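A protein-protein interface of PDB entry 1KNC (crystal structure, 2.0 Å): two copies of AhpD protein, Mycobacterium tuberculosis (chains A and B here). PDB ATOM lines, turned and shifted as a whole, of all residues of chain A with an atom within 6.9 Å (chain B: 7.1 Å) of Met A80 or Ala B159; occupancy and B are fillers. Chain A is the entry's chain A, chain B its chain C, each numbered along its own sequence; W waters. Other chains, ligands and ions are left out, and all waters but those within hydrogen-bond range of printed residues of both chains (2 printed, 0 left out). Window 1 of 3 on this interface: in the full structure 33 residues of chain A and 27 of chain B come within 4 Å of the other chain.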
ATOM      1  N   ARG A  47     -12.015  29.744   9.066  1.00  0.00           N
ATOM      2  CA  ARG A  47     -11.988  28.884  10.248  1.00  0.00           C
ATOM      3  C   ARG A  47     -11.430  29.593  11.489  1.00  0.00           C
ATOM      4  O   ARG A  47     -11.226  28.973  12.536  1.00  0.00           O
ATOM      5  CB  ARG A  47     -11.187  27.601   9.972  1.00  0.00           C
ATOM      6  CG  ARG A  47     -11.512  26.864   8.647  1.00  0.00           C
ATOM      7  CD  ARG A  47     -13.019  26.745   8.347  1.00  0.00           C
ATOM      8  NE  ARG A  47     -13.377  25.517   7.615  1.00  0.00           N
ATOM      9  CZ  ARG A  47     -13.375  25.356   6.291  1.00  0.00           C
ATOM     10  NH1 ARG A  47     -13.034  26.348   5.478  1.00  0.00           N
ATOM     11  NH2 ARG A  47     -13.722  24.178   5.781  1.00  0.00           N
ATOM     12  N   ALA A  75     -21.206  29.135   3.265  1.00  0.00           N
ATOM     13  CA  ALA A  75     -19.887  28.682   3.694  1.00  0.00           C
ATOM     14  C   ALA A  75     -19.933  27.186   4.017  1.00  0.00           C
ATOM     15  O   ALA A  75     -19.024  26.436   3.661  1.00  0.00           O
ATOM     16  CB  ALA A  75     -19.424  29.476   4.928  1.00  0.00           C
ATOM     17  N   ALA A  76     -20.994  26.757   4.694  1.00  0.00           N
ATOM     18  CA  ALA A  76     -21.148  25.353   5.065  1.00  0.00           C
ATOM     19  C   ALA A  76     -21.308  24.436   3.854  1.00  0.00           C
ATOM     20  O   ALA A  76     -20.618  23.419   3.737  1.00  0.00           O
ATOM     21  CB  ALA A  76     -22.347  25.188   5.995  1.00  0.00           C
ATOM     22  N   ILE A  77     -22.214  24.793   2.951  1.00  0.00           N
ATOM     23  CA  ILE A  77     -22.453  23.958   1.782  1.00  0.00           C
ATOM     24  C   ILE A  77     -21.226  23.905   0.861  1.00  0.00           C
ATOM     25  O   ILE A  77     -20.910  22.848   0.314  1.00  0.00           O
ATOM     26  CB  ILE A  77     -23.722  24.428   1.000  1.00  0.00           C
ATOM     27  CG1 ILE A  77     -24.214  23.309   0.080  1.00  0.00           C
ATOM     28  CG2 ILE A  77     -23.430  25.677   0.190  1.00  0.00           C
ATOM     29  CD1 ILE A  77     -24.773  22.112   0.845  1.00  0.00           C
ATOM     30  N   MET A  78     -20.537  25.032   0.689  1.00  0.00           N
ATOM     31  CA  MET A  78     -19.333  25.055  -0.144  1.00  0.00           C
ATOM     32  C   MET A  78     -18.204  24.255   0.514  1.00  0.00           C
ATOM     33  O   MET A  78     -17.297  23.773  -0.164  1.00  0.00           O
ATOM     34  CB  MET A  78     -18.860  26.490  -0.394  1.00  0.00           C
ATOM     35  CG  MET A  78     -19.719  27.269  -1.387  1.00  0.00           C
ATOM     36  SD  MET A  78     -19.828  26.450  -3.020  1.00  0.00           S
ATOM     37  CE  MET A  78     -21.446  25.715  -2.891  1.00  0.00           C
ATOM     38  N   GLY A  79     -18.255  24.129   1.836  1.00  0.00           N
ATOM     39  CA  GLY A  79     -17.240  23.368   2.543  1.00  0.00           C
ATOM     40  C   GLY A  79     -17.233  21.926   2.061  1.00  0.00           C
ATOM     41  O   GLY A  79     -16.185  21.268   2.003  1.00  0.00           O
ATOM     42  N   MET A  80     -18.422  21.434   1.720  1.00  0.00           N
ATOM     43  CA  MET A  80     -18.576  20.072   1.225  1.00  0.00           C
ATOM     44  C   MET A  80     -18.311  20.051  -0.274  1.00  0.00           C
ATOM     45  O   MET A  80     -17.435  19.328  -0.756  1.00  0.00           O
ATOM     46  CB  MET A  80     -19.988  19.542   1.510  1.00  0.00           C
ATOM     47  CG  MET A  80     -20.337  18.243   0.782  1.00  0.00           C
ATOM     48  SD  MET A  80     -22.046  17.716   1.089  1.00  0.00           S
ATOM     49  CE  MET A  80     -22.965  18.848   0.033  1.00  0.00           C
ATOM     50  N   ASN A  81     -19.053  20.870  -1.010  1.00  0.00           N
ATOM     51  CA  ASN A  81     -18.910  20.944  -2.460  1.00  0.00           C
ATOM     52  C   ASN A  81     -17.501  21.240  -2.955  1.00  0.00           C
ATOM     53  O   ASN A  81     -17.054  20.647  -3.944  1.00  0.00           O
ATOM     54  CB  ASN A  81     -19.887  21.991  -3.018  1.00  0.00           C
ATOM     55  CG  ASN A  81     -21.320  21.489  -3.049  1.00  0.00           C
ATOM     56  OD1 ASN A  81     -21.702  20.634  -2.255  1.00  0.00           O
ATOM     57  ND2 ASN A  81     -22.122  22.025  -3.961  1.00  0.00           N
ATOM     58  N   ASN A  82     -16.799  22.160  -2.297  1.00  0.00           N
ATOM     59  CA  ASN A  82     -15.440  22.509  -2.733  1.00  0.00           C
ATOM     60  C   ASN A  82     -14.502  21.286  -2.717  1.00  0.00           C
ATOM     61  O   ASN A  82     -13.680  21.125  -3.619  1.00  0.00           O
ATOM     62  CB  ASN A  82     -14.865  23.637  -1.855  1.00  0.00           C
ATOM     63  CG  ASN A  82     -15.534  25.002  -2.117  1.00  0.00           C
ATOM     64  OD1 ASN A  82     -15.297  25.963  -1.389  1.00  0.00           O
ATOM     65  ND2 ASN A  82     -16.358  25.084  -3.168  1.00  0.00           N
ATOM     66  N   VAL A  83     -14.629  20.438  -1.701  1.00  0.00           N
ATOM     67  CA  VAL A  83     -13.805  19.239  -1.600  1.00  0.00           C
ATOM     68  C   VAL A  83     -14.217  18.211  -2.661  1.00  0.00           C
ATOM     69  O   VAL A  83     -13.379  17.702  -3.413  1.00  0.00           O
ATOM     70  CB  VAL A  83     -13.920  18.598  -0.191  1.00  0.00           C
ATOM     71  CG1 VAL A  83     -13.175  17.245  -0.144  1.00  0.00           C
ATOM     72  CG2 VAL A  83     -13.330  19.551   0.855  1.00  0.00           C
ATOM     73  N   PHE A  84     -15.515  17.919  -2.720  1.00  0.00           N
ATOM     74  CA  PHE A  84     -16.044  16.942  -3.674  1.00  0.00           C
ATOM     75  C   PHE A  84     -15.694  17.245  -5.121  1.00  0.00           C
ATOM     76  O   PHE A  84     -15.144  16.396  -5.827  1.00  0.00           O
ATOM     77  CB  PHE A  84     -17.572  16.823  -3.566  1.00  0.00           C
ATOM     78  CG  PHE A  84     -18.175  15.920  -4.620  1.00  0.00           C
ATOM     79  CD1 PHE A  84     -18.140  14.535  -4.473  1.00  0.00           C
ATOM     80  CD2 PHE A  84     -18.703  16.455  -5.793  1.00  0.00           C
ATOM     81  CE1 PHE A  84     -18.617  13.694  -5.480  1.00  0.00           C
ATOM     82  CE2 PHE A  84     -19.184  15.624  -6.810  1.00  0.00           C
ATOM     83  CZ  PHE A  84     -19.138  14.238  -6.651  1.00  0.00           C
ATOM     84  N   TYR A  85     -16.024  18.448  -5.576  1.00  0.00           N
ATOM     85  CA  TYR A  85     -15.749  18.822  -6.953  1.00  0.00           C
ATOM     86  C   TYR A  85     -14.277  19.029  -7.248  1.00  0.00           C
ATOM     87  O   TYR A  85     -13.838  18.878  -8.389  1.00  0.00           O
ATOM     88  CB  TYR A  85     -16.539  20.071  -7.320  1.00  0.00           C
ATOM     89  CG  TYR A  85     -18.009  19.781  -7.497  1.00  0.00           C
ATOM     90  CD1 TYR A  85     -18.459  19.017  -8.576  1.00  0.00           C
ATOM     91  CD2 TYR A  85     -18.946  20.218  -6.561  1.00  0.00           C
ATOM     92  CE1 TYR A  85     -19.800  18.689  -8.715  1.00  0.00           C
ATOM     93  CE2 TYR A  85     -20.288  19.895  -6.691  1.00  0.00           C
ATOM     94  CZ  TYR A  85     -20.707  19.128  -7.773  1.00  0.00           C
ATOM     95  OH  TYR A  85     -22.035  18.809  -7.884  1.00  0.00           O
ATOM     96  N   ARG A  86     -13.505  19.391  -6.232  1.00  0.00           N
ATOM     97  CA  ARG A  86     -12.072  19.582  -6.442  1.00  0.00           C
ATOM     98  C   ARG A  86     -11.436  18.213  -6.694  1.00  0.00           C
ATOM     99  O   ARG A  86     -10.667  18.037  -7.641  1.00  0.00           O
ATOM    100  CB  ARG A  86     -11.421  20.251  -5.216  1.00  0.00           C
ATOM    101  CG  ARG A  86      -9.891  20.338  -5.282  1.00  0.00           C
ATOM    102  CD  ARG A  86      -9.326  21.215  -4.158  1.00  0.00           C
ATOM    103  NE  ARG A  86      -9.486  20.603  -2.847  1.00  0.00           N
ATOM    104  CZ  ARG A  86      -9.850  21.261  -1.750  1.00  0.00           C
ATOM    105  NH1 ARG A  86     -10.096  22.563  -1.807  1.00  0.00           N
ATOM    106  NH2 ARG A  86      -9.980  20.612  -0.599  1.00  0.00           N
ATOM    107  N   LEU A 102     -25.327  13.919  -3.328  1.00  0.00           N
ATOM    108  CA  LEU A 102     -25.175  14.829  -2.198  1.00  0.00           C
ATOM    109  C   LEU A 102     -26.321  15.831  -2.167  1.00  0.00           C
ATOM    110  O   LEU A 102     -26.600  16.490  -3.164  1.00  0.00           O
ATOM    111  CB  LEU A 102     -23.843  15.579  -2.300  1.00  0.00           C
ATOM    112  CG  LEU A 102     -22.571  14.724  -2.261  1.00  0.00           C
ATOM    113  CD1 LEU A 102     -21.355  15.588  -2.571  1.00  0.00           C
ATOM    114  CD2 LEU A 102     -22.440  14.071  -0.894  1.00  0.00           C
ATOM    115  N   ARG A 103     -26.981  15.941  -1.022  1.00  0.00           N
ATOM    116  CA  ARG A 103     -28.081  16.880  -0.883  1.00  0.00           C
ATOM    117  C   ARG A 103     -27.537  18.305  -0.727  1.00  0.00           C
ATOM    118  O   ARG A 103     -26.662  18.551   0.099  1.00  0.00           O
ATOM    119  CB  ARG A 103     -28.923  16.507   0.336  1.00  0.00           C
ATOM    120  CG  ARG A 103     -30.222  17.279   0.477  1.00  0.00           C
ATOM    121  CD  ARG A 103     -31.062  16.669   1.585  1.00  0.00           C
ATOM    122  NE  ARG A 103     -32.460  17.094   1.550  1.00  0.00           N
ATOM    123  CZ  ARG A 103     -32.922  18.226   2.074  1.00  0.00           C
ATOM    124  NH1 ARG A 103     -32.098  19.067   2.686  1.00  0.00           N
ATOM    125  NH2 ARG A 103     -34.214  18.513   1.987  1.00  0.00           N
ATOM    126  N   MET A 104     -28.043  19.229  -1.541  1.00  0.00           N
ATOM    127  CA  MET A 104     -27.638  20.633  -1.473  1.00  0.00           C
ATOM    128  C   MET A 104     -28.836  21.514  -1.811  1.00  0.00           C
ATOM    129  O   MET A 104     -28.782  22.375  -2.691  1.00  0.00           O
ATOM    130  CB  MET A 104     -26.455  20.918  -2.411  1.00  0.00           C
ATOM    131  CG  MET A 104     -26.492  20.158  -3.715  1.00  0.00           C
ATOM    132  SD  MET A 104     -25.031  20.384  -4.749  1.00  0.00           S
ATOM    133  CE  MET A 104     -24.009  19.013  -4.195  1.00  0.00           C
ATOM    134  N   ASN A 128     -11.377  28.393  -0.242  1.00  0.00           N
ATOM    135  CA  ASN A 128     -11.073  26.970  -0.129  1.00  0.00           C
ATOM    136  C   ASN A 128     -10.200  26.530  -1.300  1.00  0.00           C
ATOM    137  O   ASN A 128      -9.431  25.578  -1.194  1.00  0.00           O
ATOM    138  CB  ASN A 128     -12.354  26.132  -0.114  1.00  0.00           C
ATOM    139  CG  ASN A 128     -13.129  26.285   1.173  1.00  0.00           C
ATOM    140  OD1 ASN A 128     -12.536  26.414   2.243  1.00  0.00           O
ATOM    141  ND2 ASN A 128     -14.458  26.263   1.082  1.00  0.00           N
ATOM    142  N   CYS A 133     -15.871  24.792  -8.663  1.00  0.00           N
ATOM    143  CA  CYS A 133     -16.891  25.611  -8.050  1.00  0.00           C
ATOM    144  C   CYS A 133     -16.734  27.107  -8.324  1.00  0.00           C
ATOM    145  O   CYS A 133     -17.726  27.797  -8.545  1.00  0.00           O
ATOM    146  CB  CYS A 133     -16.936  25.339  -6.543  1.00  0.00           C
ATOM    147  SG  CYS A 133     -17.318  23.615  -6.111  1.00  0.00           S
ATOM    148  N   ASP B  16     -28.696  20.351   4.975  1.00  0.00           N
ATOM    149  CA  ASP B  16     -28.198  19.484   3.911  1.00  0.00           C
ATOM    150  C   ASP B  16     -27.035  18.634   4.426  1.00  0.00           C
ATOM    151  O   ASP B  16     -26.987  17.428   4.191  1.00  0.00           O
ATOM    152  CB  ASP B  16     -27.724  20.307   2.708  1.00  0.00           C
ATOM    153  CG  ASP B  16     -28.874  20.893   1.906  1.00  0.00           C
ATOM    154  OD1 ASP B  16     -29.732  20.108   1.434  1.00  0.00           O
ATOM    155  OD2 ASP B  16     -28.911  22.133   1.738  1.00  0.00           O
ATOM    156  N   ILE B  17     -26.099  19.275   5.121  1.00  0.00           N
ATOM    157  CA  ILE B  17     -24.938  18.577   5.663  1.00  0.00           C
ATOM    158  C   ILE B  17     -25.373  17.527   6.682  1.00  0.00           C
ATOM    159  O   ILE B  17     -24.868  16.407   6.673  1.00  0.00           O
ATOM    160  CB  ILE B  17     -23.940  19.562   6.348  1.00  0.00           C
ATOM    161  CG1 ILE B  17     -23.483  20.632   5.351  1.00  0.00           C
ATOM    162  CG2 ILE B  17     -22.714  18.805   6.864  1.00  0.00           C
ATOM    163  CD1 ILE B  17     -22.835  20.078   4.099  1.00  0.00           C
ATOM    164  N   ASN B  20     -26.723  14.547   4.845  1.00  0.00           N
ATOM    165  CA  ASN B  20     -25.687  13.821   4.114  1.00  0.00           C
ATOM    166  C   ASN B  20     -24.845  12.993   5.076  1.00  0.00           C
ATOM    167  O   ASN B  20     -24.356  11.924   4.719  1.00  0.00           O
ATOM    168  CB  ASN B  20     -24.785  14.785   3.341  1.00  0.00           C
ATOM    169  CG  ASN B  20     -25.458  15.345   2.105  1.00  0.00           C
ATOM    170  OD1 ASN B  20     -26.027  14.603   1.298  1.00  0.00           O
ATOM    171  ND2 ASN B  20     -25.387  16.661   1.939  1.00  0.00           N
ATOM    172  N   SER B  42     -10.570  11.643   7.479  1.00  0.00           N
ATOM    173  CA  SER B  42     -11.164  12.894   7.024  1.00  0.00           C
ATOM    174  C   SER B  42     -11.404  13.842   8.191  1.00  0.00           C
ATOM    175  O   SER B  42     -11.079  15.031   8.122  1.00  0.00           O
ATOM    176  CB  SER B  42     -12.486  12.625   6.303  1.00  0.00           C
ATOM    177  OG  SER B  42     -12.252  11.945   5.089  1.00  0.00           O
ATOM    178  N   ALA B 123      -8.667   9.985   0.376  1.00  0.00           N
ATOM    179  CA  ALA B 123      -9.631  10.873   1.015  1.00  0.00           C
ATOM    180  C   ALA B 123      -9.006  12.161   1.565  1.00  0.00           C
ATOM    181  O   ALA B 123      -9.538  13.252   1.354  1.00  0.00           O
ATOM    182  CB  ALA B 123     -10.354  10.132   2.124  1.00  0.00           C
ATOM    183  N   ALA B 126      -7.987  14.718  -1.051  1.00  0.00           N
ATOM    184  CA  ALA B 126      -9.071  15.506  -1.642  1.00  0.00           C
ATOM    185  C   ALA B 126      -9.301  16.713  -0.743  1.00  0.00           C
ATOM    186  O   ALA B 126      -9.473  17.833  -1.222  1.00  0.00           O
ATOM    187  CB  ALA B 126     -10.352  14.668  -1.753  1.00  0.00           C
ATOM    188  N   ILE B 127      -9.289  16.476   0.564  1.00  0.00           N
ATOM    189  CA  ILE B 127      -9.476  17.550   1.525  1.00  0.00           C
ATOM    190  C   ILE B 127      -8.364  18.601   1.492  1.00  0.00           C
ATOM    191  O   ILE B 127      -8.644  19.799   1.553  1.00  0.00           O
ATOM    192  CB  ILE B 127      -9.595  16.996   2.949  1.00  0.00           C
ATOM    193  CG1 ILE B 127     -10.779  16.027   3.012  1.00  0.00           C
ATOM    194  CG2 ILE B 127      -9.776  18.156   3.944  1.00  0.00           C
ATOM    195  CD1 ILE B 127     -10.912  15.303   4.322  1.00  0.00           C
ATOM    196  N   GLU B 153     -17.141   6.767  -3.148  1.00  0.00           N
ATOM    197  CA  GLU B 153     -17.798   6.840  -1.850  1.00  0.00           C
ATOM    198  C   GLU B 153     -16.868   7.473  -0.813  1.00  0.00           C
ATOM    199  O   GLU B 153     -17.324   8.153   0.111  1.00  0.00           O
ATOM    200  CB  GLU B 153     -18.222   5.440  -1.386  1.00  0.00           C
ATOM    201  CG  GLU B 153     -19.155   5.446  -0.176  1.00  0.00           C
ATOM    202  CD  GLU B 153     -20.612   5.716  -0.549  1.00  0.00           C
ATOM    203  OE1 GLU B 153     -20.857   6.266  -1.645  1.00  0.00           O
ATOM    204  OE2 GLU B 153     -21.506   5.385   0.261  1.00  0.00           O
ATOM    205  N   ALA B 154     -15.567   7.245  -0.963  1.00  0.00           N
ATOM    206  CA  ALA B 154     -14.586   7.817  -0.041  1.00  0.00           C
ATOM    207  C   ALA B 154     -14.521   9.333  -0.246  1.00  0.00           C
ATOM    208  O   ALA B 154     -14.415  10.091   0.718  1.00  0.00           O
ATOM    209  CB  ALA B 154     -13.201   7.190  -0.276  1.00  0.00           C
ATOM    210  N   LEU B 155     -14.571   9.764  -1.504  1.00  0.00           N
ATOM    211  CA  LEU B 155     -14.539  11.187  -1.824  1.00  0.00           C
ATOM    212  C   LEU B 155     -15.754  11.877  -1.205  1.00  0.00           C
ATOM    213  O   LEU B 155     -15.639  12.955  -0.605  1.00  0.00           O
ATOM    214  CB  LEU B 155     -14.537  11.404  -3.340  1.00  0.00           C
ATOM    215  CG  LEU B 155     -14.612  12.860  -3.814  1.00  0.00           C
ATOM    216  CD1 LEU B 155     -13.386  13.631  -3.332  1.00  0.00           C
ATOM    217  CD2 LEU B 155     -14.684  12.905  -5.336  1.00  0.00           C
ATOM    218  N   LYS B 156     -16.919  11.257  -1.348  1.00  0.00           N
ATOM    219  CA  LYS B 156     -18.143  11.814  -0.788  1.00  0.00           C
ATOM    220  C   LYS B 156     -18.050  11.963   0.731  1.00  0.00           C
ATOM    221  O   LYS B 156     -18.421  12.996   1.285  1.00  0.00           O
ATOM    222  CB  LYS B 156     -19.341  10.928  -1.147  1.00  0.00           C
ATOM    223  CG  LYS B 156     -19.804  11.055  -2.606  1.00  0.00           C
ATOM    224  CD  LYS B 156     -20.808   9.958  -2.993  1.00  0.00           C
ATOM    225  CE  LYS B 156     -22.022   9.908  -2.063  1.00  0.00           C
ATOM    226  NZ  LYS B 156     -23.090   9.031  -2.617  1.00  0.00           N
ATOM    227  N   ALA B 157     -17.542  10.934   1.402  1.00  0.00           N
ATOM    228  CA  ALA B 157     -17.419  10.966   2.857  1.00  0.00           C
ATOM    229  C   ALA B 157     -16.459  12.060   3.314  1.00  0.00           C
ATOM    230  O   ALA B 157     -16.676  12.697   4.348  1.00  0.00           O
ATOM    231  CB  ALA B 157     -16.947   9.609   3.371  1.00  0.00           C
ATOM    232  N   ALA B 158     -15.388  12.259   2.553  1.00  0.00           N
ATOM    233  CA  ALA B 158     -14.401  13.289   2.878  1.00  0.00           C
ATOM    234  C   ALA B 158     -15.064  14.655   2.752  1.00  0.00           C
ATOM    235  O   ALA B 158     -14.959  15.502   3.646  1.00  0.00           O
ATOM    236  CB  ALA B 158     -13.214  13.201   1.924  1.00  0.00           C
ATOM    237  N   ALA B 159     -15.748  14.858   1.632  1.00  0.00           N
ATOM    238  CA  ALA B 159     -16.438  16.110   1.386  1.00  0.00           C
ATOM    239  C   ALA B 159     -17.477  16.390   2.465  1.00  0.00           C
ATOM    240  O   ALA B 159     -17.540  17.495   2.998  1.00  0.00           O
ATOM    241  CB  ALA B 159     -17.101  16.086   0.017  1.00  0.00           C
ATOM    242  N   ILE B 160     -18.283  15.385   2.800  1.00  0.00           N
ATOM    243  CA  ILE B 160     -19.325  15.562   3.811  1.00  0.00           C
ATOM    244  C   ILE B 160     -18.748  15.923   5.176  1.00  0.00           C
ATOM    245  O   ILE B 160     -19.241  16.835   5.845  1.00  0.00           O
ATOM    246  CB  ILE B 160     -20.198  14.291   3.949  1.00  0.00           C
ATOM    247  CG1 ILE B 160     -20.983  14.062   2.655  1.00  0.00           C
ATOM    248  CG2 ILE B 160     -21.172  14.441   5.113  1.00  0.00           C
ATOM    249  CD1 ILE B 160     -21.644  12.700   2.572  1.00  0.00           C
ATOM    250  N   VAL B 161     -17.709  15.210   5.599  1.00  0.00           N
ATOM    251  CA  VAL B 161     -17.090  15.501   6.892  1.00  0.00           C
ATOM    252  C   VAL B 161     -16.550  16.937   6.891  1.00  0.00           C
ATOM    253  O   VAL B 161     -16.593  17.646   7.913  1.00  0.00           O
ATOM    254  CB  VAL B 161     -15.949  14.500   7.201  1.00  0.00           C
ATOM    255  CG1 VAL B 161     -15.192  14.939   8.453  1.00  0.00           C
ATOM    256  CG2 VAL B 161     -16.530  13.112   7.400  1.00  0.00           C
ATOM    257  N   SER B 162     -16.048  17.365   5.736  1.00  0.00           N
ATOM    258  CA  SER B 162     -15.519  18.723   5.584  1.00  0.00           C
ATOM    259  C   SER B 162     -16.646  19.732   5.775  1.00  0.00           C
ATOM    260  O   SER B 162     -16.446  20.804   6.348  1.00  0.00           O
ATOM    261  CB  SER B 162     -14.898  18.909   4.194  1.00  0.00           C
ATOM    262  OG  SER B 162     -13.785  18.044   4.015  1.00  0.00           O
ATOM    263  N   GLY B 163     -17.830  19.385   5.280  1.00  0.00           N
ATOM    264  CA  GLY B 163     -18.971  20.270   5.421  1.00  0.00           C
ATOM    265  C   GLY B 163     -19.383  20.350   6.876  1.00  0.00           C
ATOM    266  O   GLY B 163     -19.782  21.408   7.360  1.00  0.00           O
ATOM    267  N   VAL B 164     -19.293  19.220   7.571  1.00  0.00           N
ATOM    268  CA  VAL B 164     -19.650  19.160   8.984  1.00  0.00           C
ATOM    269  C   VAL B 164     -18.719  20.055   9.809  1.00  0.00           C
ATOM    270  O   VAL B 164     -19.174  20.875  10.601  1.00  0.00           O
ATOM    271  CB  VAL B 164     -19.554  17.713   9.534  1.00  0.00           C
ATOM    272  CG1 VAL B 164     -19.851  17.703  11.028  1.00  0.00           C
ATOM    273  CG2 VAL B 164     -20.540  16.809   8.806  1.00  0.00           C
ATOM    274  N   ALA B 165     -17.418  19.881   9.612  1.00  0.00           N
ATOM    275  CA  ALA B 165     -16.418  20.652  10.332  1.00  0.00           C
ATOM    276  C   ALA B 165     -16.631  22.152  10.136  1.00  0.00           C
ATOM    277  O   ALA B 165     -16.548  22.930  11.086  1.00  0.00           O
ATOM    278  CB  ALA B 165     -15.024  20.251   9.876  1.00  0.00           C
ATOM    279  N   GLN B 166     -16.895  22.554   8.897  1.00  0.00           N
ATOM    280  CA  GLN B 166     -17.131  23.960   8.594  1.00  0.00           C
ATOM    281  C   GLN B 166     -18.390  24.450   9.297  1.00  0.00           C
ATOM    282  O   GLN B 166     -18.392  25.515   9.917  1.00  0.00           O
ATOM    283  CB  GLN B 166     -17.282  24.178   7.086  1.00  0.00           C
ATOM    284  CG  GLN B 166     -17.796  25.570   6.707  1.00  0.00           C
ATOM    285  CD  GLN B 166     -16.781  26.675   6.963  1.00  0.00           C
ATOM    286  OE1 GLN B 166     -15.813  26.837   6.216  1.00  0.00           O
ATOM    287  NE2 GLN B 166     -17.001  27.441   8.019  1.00  0.00           N
HETATM  288  O   HOH W   1     -16.133  26.410   3.682  1.00  0.00           O
HETATM  289  O   HOH W   2     -13.906  21.766   6.542  1.00  0.00           O
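Water W2 bridges the guanidinium group (NH2) of Arg A47 (2.5 Å) and the backbone carbonyl oxygen (O) of Ser B162 (2.7 Å). Water W1 lies within hydrogen-bond range of OE1 of Gln B166, O of Ala A75 and ND2 of Asn A128.
NH1 of Arg A103 lies within salt-bridge range of OD1 of Asp B16 (2.9 Å). NH1 of Arg A47 sits close to OE1 of Gln B166. The side-chain sulfur (SD) of Met A80 sits at hydrogen-bond distance from the side-chain amide nitrogen (ND2) of Asn B20, at 3.6 Å. The guanidinium group (NH2) of Arg A86 lies within hydrogen-bond range of the backbone carbonyl oxygen (O) of Ala B126, 2.9 Å away. O of Ile B127 is in hydrogen-bond range of NH2 of Arg A86, at 2.7 Å. The backbone NH (N) of Arg A103 sits at hydrogen-bond distance from the side-chain amide oxygen (OD1) of Asn B20.
ND2 of Asn B20 lies within hydrogen-bond range of O of Asp B16, 2.9 Å away. The backbone carbonyl oxygen (O) of Ala B158 lies within hydrogen-bond range of the side-chain hydroxyl (OG) of Ser B162 (2.8 Å). The guanidinium group (NH1) of Arg A47 lies within hydrogen-bond range of the side-chain amide oxygen (OD1) of Asn A128, 3.3 Å away. The side-chain amide nitrogen of Asn A81 is in hydrogen-bond range of the side-chain sulfur of Met A104 (3.4 Å). NH1 of Arg A86 is in hydrogen-bond range of O of Asn A128 (3.1 Å). The side-chain amide oxygen (OD1) of Asn A81 sits close to the backbone carbonyl oxygen (O) of Ile A77, 3.5 Å away.
Hydrophobic or aromatic side chains of chain A within 4 Å of the printed part of chain B: Ile A77, Met A80, Val A83, Phe A84 and Leu A102. Of the 21 printed residues of chain B, 11 touch a printed residue of chain A. Printed residues of chain B that touch a printed residue of chain A: Asp B16, Ile B17, Asn B20, Ala B126, Ile B127, Leu B155, Ala B159, Ile B160, Ser B162, Gly B163 and Gln B166. Hydrophobic or aromatic side chains of chain B that line the printed part of chain A: Ile B17, Leu B155, Ala B159 and Ile B160. Along chain B the printed residues that touch a printed residue of chain A span positions 16 to 166. Among the printed residues, 22 pairs touch across the chains.
No position is printed for both chains.
Among the printed residues, pairs that only touch across the chains: Ala A75 with Gln B166, Ala A76 with Gly B163, Ala A76 with Gln B166, Ile A77 with Asp B16, Gly A79 with Ser B162, Met A80 with Ile B17, Met A80 with Ala B159, Met A80 with Gly B163, Val A83 with Ala B126, Val A83 with Ala B159, Val A83 with Ser B162, Phe A84 with Leu B155, Phe A84 with Ala B159, Leu A102 with Asn B20, Leu A102 with Ile B160 and Met A104 with Asp B16.
Of chain B, only Ile B17 (3.9 Å), Asn B20 (3.6 Å), Ala B159 (3.3 Å) and Gly B163 (3.9 Å) come within 4 Å of Met A80. Ala B159 touches three residues of chain A. Gly A79 touches just one residue of chain B: Ser B162. Of the printed residues of chain A, Ile B17 touches Met A80. Printed residues of chain A within 4 Å of Ile B127: Arg A86. Of the printed residues of chain A, Ala B126 touches Val A83 and Arg A86. Ala B157 touches none of the printed residues of chain A. Met A78 touches none of the printed residues of chain B.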
